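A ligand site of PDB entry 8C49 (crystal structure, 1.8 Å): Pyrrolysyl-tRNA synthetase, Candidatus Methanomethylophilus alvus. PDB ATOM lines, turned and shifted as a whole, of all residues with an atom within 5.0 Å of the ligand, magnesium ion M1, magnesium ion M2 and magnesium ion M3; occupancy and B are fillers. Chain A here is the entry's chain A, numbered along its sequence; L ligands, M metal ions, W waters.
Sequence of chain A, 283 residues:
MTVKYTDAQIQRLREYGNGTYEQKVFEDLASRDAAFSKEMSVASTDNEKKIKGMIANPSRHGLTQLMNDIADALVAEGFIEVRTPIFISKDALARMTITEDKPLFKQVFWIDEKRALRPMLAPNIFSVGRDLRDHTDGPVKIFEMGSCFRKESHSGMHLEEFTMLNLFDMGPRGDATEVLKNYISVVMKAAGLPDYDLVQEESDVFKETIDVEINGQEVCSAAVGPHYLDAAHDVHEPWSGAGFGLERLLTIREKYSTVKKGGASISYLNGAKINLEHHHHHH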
ATOM      1  N   GLN A 107      -3.363  16.367  -5.365  1.00  0.00           N
ATOM      2  CA  GLN A 107      -4.672  16.979  -5.173  1.00  0.00           C
ATOM      3  C   GLN A 107      -5.707  16.004  -4.650  1.00  0.00           C
ATOM      4  O   GLN A 107      -6.865  16.397  -4.460  1.00  0.00           O
ATOM      5  CB  GLN A 107      -5.167  17.567  -6.503  1.00  0.00           C
ATOM      6  CG  GLN A 107      -4.176  18.510  -7.165  1.00  0.00           C
ATOM      7  CD  GLN A 107      -4.776  19.222  -8.361  1.00  0.00           C
ATOM      8  OE1 GLN A 107      -4.477  18.892  -9.511  1.00  0.00           O
ATOM      9  NE2 GLN A 107      -5.643  20.197  -8.105  1.00  0.00           N
ATOM     10  N   MET A 120     -11.835  12.300 -10.551  1.00  0.00           N
ATOM     11  CA  MET A 120     -12.407  12.253 -11.876  1.00  0.00           C
ATOM     12  C   MET A 120     -13.269  11.001 -11.962  1.00  0.00           C
ATOM     13  O   MET A 120     -13.157  10.088 -11.140  1.00  0.00           O
ATOM     14  CB  MET A 120     -11.322  12.268 -12.962  1.00  0.00           C
ATOM     15  CG  MET A 120     -10.167  11.312 -12.693  1.00  0.00           C
ATOM     16  SD  MET A 120      -9.162  10.976 -14.161  1.00  0.00           S
ATOM     17  CE  MET A 120      -8.256  12.514 -14.310  1.00  0.00           C
ATOM     18  N   ARG A 150     -10.892  17.668  -5.627  1.00  0.00           N
ATOM     19  CA  ARG A 150      -9.487  17.985  -5.834  1.00  0.00           C
ATOM     20  C   ARG A 150      -9.092  19.112  -4.891  1.00  0.00           C
ATOM     21  O   ARG A 150      -9.842  20.080  -4.716  1.00  0.00           O
ATOM     22  CB  ARG A 150      -9.206  18.412  -7.284  1.00  0.00           C
ATOM     23  CG  ARG A 150      -9.308  17.303  -8.300  1.00  0.00           C
ATOM     24  CD  ARG A 150      -9.116  17.842  -9.702  1.00  0.00           C
ATOM     25  NE  ARG A 150      -9.572  16.891 -10.713  1.00  0.00           N
ATOM     26  CZ  ARG A 150      -9.227  16.918 -11.990  1.00  0.00           C
ATOM     27  NH1 ARG A 150      -8.414  17.852 -12.468  1.00  0.00           N
ATOM     28  NH2 ARG A 150      -9.685  15.982 -12.809  1.00  0.00           N
ATOM     29  N   GLU A 152      -7.361  22.380  -4.364  1.00  0.00           N
ATOM     30  CA  GLU A 152      -7.106  23.472  -5.285  1.00  0.00           C
ATOM     31  C   GLU A 152      -6.743  24.736  -4.517  1.00  0.00           C
ATOM     32  O   GLU A 152      -7.144  24.919  -3.368  1.00  0.00           O
ATOM     33  CB  GLU A 152      -8.337  23.757  -6.167  1.00  0.00           C
ATOM     34  CG  GLU A 152      -8.891  22.545  -6.903  1.00  0.00           C
ATOM     35  CD  GLU A 152      -8.099  22.225  -8.160  1.00  0.00           C
ATOM     36  OE1 GLU A 152      -7.078  22.887  -8.404  1.00  0.00           O
ATOM     37  OE2 GLU A 152      -8.523  21.315  -8.910  1.00  0.00           O
ATOM     38  N   MET A 157     -12.301  29.800 -10.871  1.00  0.00           N
ATOM     39  CA  MET A 157     -12.884  28.696 -11.638  1.00  0.00           C
ATOM     40  C   MET A 157     -12.478  27.320 -11.106  1.00  0.00           C
ATOM     41  O   MET A 157     -12.538  26.337 -11.857  1.00  0.00           O
ATOM     42  CB  MET A 157     -12.531  28.798 -13.115  1.00  0.00           C
ATOM     43  CG  MET A 157     -12.853  30.160 -13.714  1.00  0.00           C
ATOM     44  SD  MET A 157     -14.435  30.137 -14.579  1.00  0.00           S
ATOM     45  CE  MET A 157     -14.190  28.858 -15.788  1.00  0.00           C
ATOM     46  N   HIS A 158     -12.135  27.231  -9.829  1.00  0.00           N
ATOM     47  CA  HIS A 158     -11.844  25.951  -9.208  1.00  0.00           C
ATOM     48  C   HIS A 158     -12.639  25.820  -7.916  1.00  0.00           C
ATOM     49  O   HIS A 158     -12.751  26.777  -7.136  1.00  0.00           O
ATOM     50  CB  HIS A 158     -10.361  25.797  -8.913  1.00  0.00           C
ATOM     51  CG  HIS A 158      -9.526  25.544 -10.128  1.00  0.00           C
ATOM     52  ND1 HIS A 158      -9.056  26.559 -10.941  1.00  0.00           N
ATOM     53  CD2 HIS A 158      -9.079  24.394 -10.672  1.00  0.00           C
ATOM     54  CE1 HIS A 158      -8.357  26.035 -11.927  1.00  0.00           C
ATOM     55  NE2 HIS A 158      -8.352  24.727 -11.789  1.00  0.00           N
ATOM     56  N   LEU A 159     -13.203  24.634  -7.719  1.00  0.00           N
ATOM     57  CA  LEU A 159     -13.851  24.244  -6.474  1.00  0.00           C
ATOM     58  C   LEU A 159     -13.196  22.973  -5.972  1.00  0.00           C
ATOM     59  O   LEU A 159     -12.687  22.166  -6.752  1.00  0.00           O
ATOM     60  CB  LEU A 159     -15.352  24.004  -6.671  1.00  0.00           C
ATOM     61  CG  LEU A 159     -16.150  25.091  -7.378  1.00  0.00           C
ATOM     62  CD1 LEU A 159     -17.311  24.487  -8.144  1.00  0.00           C
ATOM     63  CD2 LEU A 159     -16.648  26.108  -6.363  1.00  0.00           C
ATOM     64  N   PHE A 162     -16.475  19.767  -7.389  1.00  0.00           N
ATOM     65  CA  PHE A 162     -17.130  20.200  -8.622  1.00  0.00           C
ATOM     66  C   PHE A 162     -17.883  19.018  -9.216  1.00  0.00           C
ATOM     67  O   PHE A 162     -17.761  17.880  -8.755  1.00  0.00           O
ATOM     68  CB  PHE A 162     -16.116  20.763  -9.619  1.00  0.00           C
ATOM     69  CG  PHE A 162     -15.081  19.774 -10.080  1.00  0.00           C
ATOM     70  CD1 PHE A 162     -14.003  19.444  -9.265  1.00  0.00           C
ATOM     71  CD2 PHE A 162     -15.182  19.185 -11.322  1.00  0.00           C
ATOM     72  CE1 PHE A 162     -13.055  18.535  -9.690  1.00  0.00           C
ATOM     73  CE2 PHE A 162     -14.239  18.273 -11.754  1.00  0.00           C
ATOM     74  CZ  PHE A 162     -13.169  17.948 -10.936  1.00  0.00           C
ATOM     75  N   MET A 164     -18.609  16.753 -12.386  1.00  0.00           N
ATOM     76  CA  MET A 164     -18.156  16.236 -13.675  1.00  0.00           C
ATOM     77  C   MET A 164     -19.297  15.603 -14.442  1.00  0.00           C
ATOM     78  O   MET A 164     -20.159  14.934 -13.873  1.00  0.00           O
ATOM     79  CB  MET A 164     -17.054  15.190 -13.470  1.00  0.00           C
ATOM     80  CG  MET A 164     -16.099  15.016 -14.650  1.00  0.00           C
ATOM     81  SD  MET A 164     -14.990  16.399 -14.948  1.00  0.00           S
ATOM     82  CE  MET A 164     -13.573  15.867 -13.988  1.00  0.00           C
ATOM     83  N   ASP A 211      -9.232  19.635 -25.567  1.00  0.00           N
ATOM     84  CA  ASP A 211      -9.962  20.442 -24.603  1.00  0.00           C
ATOM     85  C   ASP A 211     -10.997  21.299 -25.320  1.00  0.00           C
ATOM     86  O   ASP A 211     -10.763  21.784 -26.435  1.00  0.00           O
ATOM     87  CB  ASP A 211      -9.012  21.341 -23.814  1.00  0.00           C
ATOM     88  CG  ASP A 211      -8.288  20.594 -22.703  1.00  0.00           C
ATOM     89  OD1 ASP A 211      -8.330  19.340 -22.703  1.00  0.00           O
ATOM     90  OD2 ASP A 211      -7.671  21.247 -21.849  1.00  0.00           O
ATOM     91  N   GLN A 217     -11.185  29.482 -22.042  1.00  0.00           N
ATOM     92  CA  GLN A 217     -11.370  28.895 -20.728  1.00  0.00           C
ATOM     93  C   GLN A 217     -11.779  27.441 -20.870  1.00  0.00           C
ATOM     94  O   GLN A 217     -12.781  27.129 -21.522  1.00  0.00           O
ATOM     95  CB  GLN A 217     -12.402  29.683 -19.922  1.00  0.00           C
ATOM     96  CG  GLN A 217     -12.819  28.961 -18.694  1.00  0.00           C
ATOM     97  CD  GLN A 217     -11.699  28.972 -17.677  1.00  0.00           C
ATOM     98  OE1 GLN A 217     -11.177  30.023 -17.330  1.00  0.00           O
ATOM     99  NE2 GLN A 217     -11.358  27.791 -17.166  1.00  0.00           N
ATOM    100  N   GLU A 218     -11.029  26.561 -20.216  1.00  0.00           N
ATOM    101  CA  GLU A 218     -11.273  25.123 -20.311  1.00  0.00           C
ATOM    102  C   GLU A 218     -12.569  24.748 -19.613  1.00  0.00           C
ATOM    103  O   GLU A 218     -12.753  25.035 -18.431  1.00  0.00           O
ATOM    104  CB  GLU A 218     -10.103  24.353 -19.693  1.00  0.00           C
ATOM    105  CG  GLU A 218     -10.250  22.841 -19.756  1.00  0.00           C
ATOM    106  CD  GLU A 218      -9.209  22.131 -18.904  1.00  0.00           C
ATOM    107  OE1 GLU A 218      -8.164  22.745 -18.613  1.00  0.00           O
ATOM    108  OE2 GLU A 218      -9.456  20.967 -18.522  1.00  0.00           O
ATOM    109  N   VAL A 219     -13.460  24.083 -20.359  1.00  0.00           N
ATOM    110  CA  VAL A 219     -14.688  23.540 -19.800  1.00  0.00           C
ATOM    111  C   VAL A 219     -14.788  22.029 -19.975  1.00  0.00           C
ATOM    112  O   VAL A 219     -15.768  21.430 -19.527  1.00  0.00           O
ATOM    113  CB  VAL A 219     -15.932  24.227 -20.404  1.00  0.00           C
ATOM    114  CG1 VAL A 219     -15.856  25.731 -20.193  1.00  0.00           C
ATOM    115  CG2 VAL A 219     -16.065  23.896 -21.879  1.00  0.00           C
ATOM    116  N   CYS A 220     -13.815  21.407 -20.622  1.00  0.00           N
ATOM    117  CA  CYS A 220     -13.828  19.958 -20.839  1.00  0.00           C
ATOM    118  C   CYS A 220     -12.451  19.514 -21.292  1.00  0.00           C
ATOM    119  O   CYS A 220     -11.745  20.238 -22.001  1.00  0.00           O
ATOM    120  CB  CYS A 220     -14.872  19.560 -21.881  1.00  0.00           C
ATOM    121  SG  CYS A 220     -14.736  17.858 -22.491  1.00  0.00           S
ATOM    122  N   SER A 221     -12.080  18.305 -20.869  1.00  0.00           N
ATOM    123  CA  SER A 221     -10.903  17.610 -21.387  1.00  0.00           C
ATOM    124  C   SER A 221     -11.354  16.249 -21.887  1.00  0.00           C
ATOM    125  O   SER A 221     -12.046  15.524 -21.175  1.00  0.00           O
ATOM    126  CB  SER A 221      -9.809  17.470 -20.332  1.00  0.00           C
ATOM    127  OG  SER A 221      -9.083  18.669 -20.189  1.00  0.00           O
ATOM    128  N   GLY A 243     -14.691  14.636 -20.347  1.00  0.00           N
ATOM    129  CA  GLY A 243     -15.104  15.064 -19.030  1.00  0.00           C
ATOM    130  C   GLY A 243     -15.364  16.566 -18.961  1.00  0.00           C
ATOM    131  O   GLY A 243     -14.432  17.360 -19.126  1.00  0.00           O
ATOM    132  N   PHE A 244     -16.614  16.957 -18.731  1.00  0.00           N
ATOM    133  CA  PHE A 244     -17.016  18.359 -18.698  1.00  0.00           C
ATOM    134  C   PHE A 244     -17.137  18.846 -17.262  1.00  0.00           C
ATOM    135  O   PHE A 244     -17.618  18.120 -16.382  1.00  0.00           O
ATOM    136  CB  PHE A 244     -18.352  18.566 -19.401  1.00  0.00           C
ATOM    137  CG  PHE A 244     -18.337  18.261 -20.876  1.00  0.00           C
ATOM    138  CD1 PHE A 244     -18.336  16.949 -21.326  1.00  0.00           C
ATOM    139  CD2 PHE A 244     -18.360  19.284 -21.816  1.00  0.00           C
ATOM    140  CE1 PHE A 244     -18.338  16.666 -22.681  1.00  0.00           C
ATOM    141  CE2 PHE A 244     -18.357  19.005 -23.162  1.00  0.00           C
ATOM    142  CZ  PHE A 244     -18.350  17.696 -23.605  1.00  0.00           C
ATOM    143  N   GLY A 245     -16.734  20.094 -17.029  1.00  0.00           N
ATOM    144  CA  GLY A 245     -16.997  20.758 -15.762  1.00  0.00           C
ATOM    145  C   GLY A 245     -18.309  21.515 -15.796  1.00  0.00           C
ATOM    146  O   GLY A 245     -18.410  22.562 -16.427  1.00  0.00           O
ATOM    147  N   GLU A 247     -20.144  23.156 -13.493  1.00  0.00           N
ATOM    148  CA  GLU A 247     -20.163  24.491 -12.922  1.00  0.00           C
ATOM    149  C   GLU A 247     -19.535  25.511 -13.877  1.00  0.00           C
ATOM    150  O   GLU A 247     -20.010  26.654 -13.970  1.00  0.00           O
ATOM    151  CB  GLU A 247     -19.436  24.514 -11.578  1.00  0.00           C
ATOM    152  CG  GLU A 247     -20.169  23.813 -10.451  1.00  0.00           C
ATOM    153  CD  GLU A 247     -19.831  22.337 -10.376  1.00  0.00           C
ATOM    154  OE1 GLU A 247     -19.009  21.873 -11.190  1.00  0.00           O
ATOM    155  OE2 GLU A 247     -20.379  21.642  -9.491  1.00  0.00           O
ATOM    156  N   ARG A 248     -18.466  25.123 -14.559  1.00  0.00           N
ATOM    157  CA  ARG A 248     -17.839  26.040 -15.504  1.00  0.00           C
ATOM    158  C   ARG A 248     -18.775  26.349 -16.674  1.00  0.00           C
ATOM    159  O   ARG A 248     -18.875  27.501 -17.106  1.00  0.00           O
ATOM    160  CB  ARG A 248     -16.519  25.449 -16.017  1.00  0.00           C
ATOM    161  CG  ARG A 248     -15.417  25.464 -14.963  1.00  0.00           C
ATOM    162  CD  ARG A 248     -14.031  25.277 -15.560  1.00  0.00           C
ATOM    163  NE  ARG A 248     -13.004  25.205 -14.517  1.00  0.00           N
ATOM    164  CZ  ARG A 248     -11.744  24.853 -14.719  1.00  0.00           C
ATOM    165  NH1 ARG A 248     -11.292  24.554 -15.916  1.00  0.00           N
ATOM    166  NH2 ARG A 248     -10.914  24.802 -13.677  1.00  0.00           N
HETATM  167  P1  LIG L   1      -7.716  23.035 -14.993  1.00  0.00           P
HETATM  168  O1  LIG L   1      -6.418  23.300 -15.692  1.00  0.00           O
HETATM  169  O2  LIG L   1      -7.453  22.697 -13.472  1.00  0.00           O
HETATM  170  O3  LIG L   1      -8.636  24.315 -15.071  1.00  0.00           O
HETATM  171  P2  LIG L   1      -7.952  20.219 -15.393  1.00  0.00           P
HETATM  172  O4  LIG L   1      -7.172  19.668 -16.543  1.00  0.00           O
HETATM  173  O5  LIG L   1      -7.030  20.248 -14.138  1.00  0.00           O
HETATM  174  N1  LIG L   1      -8.525  21.749 -15.748  1.00  0.00           N
HETATM  175  P3  LIG L   1      -9.522  17.966 -15.890  1.00  0.00           P
HETATM  176  O6  LIG L   1      -8.733  16.838 -15.343  1.00  0.00           O
HETATM  177  O7  LIG L   1      -9.318  18.197 -17.389  1.00  0.00           O
HETATM  178  O8  LIG L   1      -9.194  19.317 -15.113  1.00  0.00           O
HETATM  179  O9  LIG L   1     -11.051  17.708 -15.544  1.00  0.00           O
HETATM  180  C1  LIG L   1     -12.083  17.742 -16.553  1.00  0.00           C
HETATM  181  C2  LIG L   1     -12.846  19.049 -16.479  1.00  0.00           C
HETATM  182  O10 LIG L   1     -13.365  19.220 -15.147  1.00  0.00           O
HETATM  183  C3  LIG L   1     -12.036  20.308 -16.755  1.00  0.00           C
HETATM  184  O11 LIG L   1     -11.943  20.578 -18.141  1.00  0.00           O
HETATM  185  C4  LIG L   1     -12.856  21.375 -16.023  1.00  0.00           C
HETATM  186  O12 LIG L   1     -13.927  21.879 -16.808  1.00  0.00           O
HETATM  187  C5  LIG L   1     -13.397  20.598 -14.812  1.00  0.00           C
HETATM  188  N2  LIG L   1     -12.641  20.803 -13.590  1.00  0.00           N
HETATM  189  C6  LIG L   1     -11.421  20.284 -13.260  1.00  0.00           C
HETATM  190  N3  LIG L   1     -10.985  20.634 -12.077  1.00  0.00           N
HETATM  191  C7  LIG L   1     -12.004  21.438 -11.578  1.00  0.00           C
HETATM  192  C8  LIG L   1     -12.155  22.128 -10.363  1.00  0.00           C
HETATM  193  N4  LIG L   1     -11.255  22.120  -9.379  1.00  0.00           N
HETATM  194  N5  LIG L   1     -13.298  22.843 -10.195  1.00  0.00           N
HETATM  195  C9  LIG L   1     -14.201  22.859 -11.168  1.00  0.00           C
HETATM  196  N6  LIG L   1     -14.164  22.251 -12.354  1.00  0.00           N
HETATM  197  C10 LIG L   1     -13.026  21.551 -12.500  1.00  0.00           C
HETATM  198 MG    MG M   1      -6.572  21.199 -12.508  1.00  0.00          MG
HETATM  199 MG    MG M   2      -8.170  19.282 -18.430  1.00  0.00          MG
HETATM  200 MG    MG M   3      -6.278  23.764 -17.865  1.00  0.00          MG
HETATM  201  O   HOH W   1      -4.567  24.978 -17.403  1.00  0.00           O
HETATM  202  O   HOH W   2      -4.290  19.642 -17.047  1.00  0.00           O
HETATM  203  O   HOH W   3      -4.922  17.936 -13.632  1.00  0.00           O
HETATM  204  O   HOH W   4      -5.766  24.648 -20.006  1.00  0.00           O
HETATM  205  O   HOH W   5      -4.699  21.707 -13.432  1.00  0.00           O
HETATM  206  O   HOH W   6      -5.261  22.001 -18.270  1.00  0.00           O
HETATM  207  O   HOH W   7      -5.929  22.272 -10.831  1.00  0.00           O
HETATM  208  O   HOH W   8      -6.639  20.253 -19.624  1.00  0.00           O
HETATM  209  O   HOH W   9      -8.357  20.812 -11.480  1.00  0.00           O
HETATM  210  O   HOH W  10      -5.016  25.196 -13.951  1.00  0.00           O
HETATM  211  O   HOH W  11      -6.807  17.490 -18.739  1.00  0.00           O
HETATM  212  O   HOH W  12      -6.812  15.267 -16.420  1.00  0.00           O
HETATM  213  O   HOH W  13      -7.509  25.573 -17.633  1.00  0.00           O
HETATM  214  O   HOH W  14     -16.911  22.588 -13.193  1.00  0.00           O
HETATM  215  O   HOH W  15      -5.561  19.443 -11.763  1.00  0.00           O
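The side-chain carboxylate (OE2) of Glu 152 is in hydrogen-bond range of a nitrogen (N4) of the ligand, at 2.9 Å. The guanidinium group of Arg 150 lies within salt-bridge range of an oxygen (O6) of the ligand, 2.8 Å away. A nitrogen (N5) of the ligand lies within hydrogen-bond range of the backbone NH (N) of Leu 159 (3.1 Å). An oxygen (O3) of the ligand is in salt-bridge range of the guanidinium group of Arg 248 (2.7 Å). An oxygen (O12) of the ligand is in hydrogen-bond range of the backbone NH (N) of Gly 245 (3.3 Å). N of Cys 220 is in hydrogen-bond range of O11 of the ligand. The backbone carbonyl oxygen (O) of Val 219 lies close to an oxygen (O12) of the ligand (3.3 Å). A ring nitrogen (NE2) of His 158 sits at hydrogen-bond distance from an oxygen (O3) of the ligand (3.3 Å). The backbone carbonyl oxygen (O) of Leu 159 lies within hydrogen-bond range of a nitrogen (N4) of the ligand (3.0 Å).
The backbone carbonyl oxygen of Val 219 sits at hydrogen-bond distance from the backbone NH of Gly 245. NH2 of Arg 248 lies within hydrogen-bond range of O of Met 157, 2.9 Å away. The guanidinium group (NH2) of Arg 248 sits at hydrogen-bond distance from a ring nitrogen (NE2) of His 158, 3.2 Å away. N of Gly 243 is in hydrogen-bond range of O of Ser 221. NH1 of Arg 248 is in hydrogen-bond range of O of Glu 218. NE2 of Gln 107 sits at hydrogen-bond distance from OE1 of Glu 152 (3.1 Å). O of Gly 243 lies close to SG of Cys 220, at 3.4 Å. The side-chain hydroxyl (OG) of Ser 221 sits close to the side-chain carboxylate (OD1) of Asp 211 (2.7 Å).
O10 of the ligand sits close to SD of Met 164, 3.3 Å away. Met 157 touches the ligand (O to C9, 3.9 Å). CB of Phe 162 touches C9 of the ligand (3.2 Å). Gly 243 touches the ligand. Within 4 Å of the ligand: Arg 150, Glu 152, Met 157, His 158, Leu 159, Phe 162, Met 164, Glu 218, Val 219, Cys 220, Ser 221, Gly 243, Gly 245 and Arg 248. The nearest printed residue that does not touch the ligand is Phe 244 (4.3 Å).
Residues that only touch magnesium ion M1: Arg 150. Of the 20 residues printed, 1 comes within 4 Å of magnesium ion M1. The nearest printed residue that does not touch magnesium ion M1 is His 158 (4.02 Å).
OD2 of Asp 211 touches magnesium ion M2 (3.97 Å). Within 4 Å of magnesium ion M2: Asp 211, Glu 218 and Ser 221.
One residue has an atom within 4 Å of magnesium ion M3: Glu 218.
Magnesium ion M1 is bound by O5 of the ligand (1.9 Å), O2 of the ligand (2.0 Å), water W7 (2.1 Å), water W9 (2.1 Å), water W5 (2.1 Å) and water W15 (2.2 Å). Magnesium ion M1 has six donor atoms within binding distance.
Magnesium ion M2 is bound by O7 of the ligand (1.9 Å), OG of Ser 221 (2.1 Å), OE2 of Glu 218 (2.1 Å), O4 of the ligand (2.2 Å), water W8 (2.2 Å) and water W11 (2.3 Å).
Magnesium ion M3 is bound by water W6 (2.1 Å), water W1 (2.1 Å), water W13 (2.2 Å), O1 of the ligand (2.2 Å), OE1 of Glu 218 (2.3 Å) and water W4 (2.4 Å). Magnesium ion M3 has six donor atoms within binding distance.
Water W9 lies within hydrogen-bond range of the side-chain carboxylate of Glu 152 (2.6 Å), a nitrogen (N3) of the ligand (2.7 Å) and the guanidinium group of Arg 150 (3.1 Å). Water W15 bridges the side-chain amide oxygen (OE1) of Gln 107 and the guanidinium group (NH1) of Arg 150. Water W7 lies within hydrogen-bond range of OE1 of Glu 152 (2.8 Å) and NE2 of Gln 107 (3.4 Å). Water W14 lies within hydrogen-bond range of N6 of the ligand (2.9 Å), OE1 of Glu 247 (3.0 Å) and N of Arg 248 (3.3 Å).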
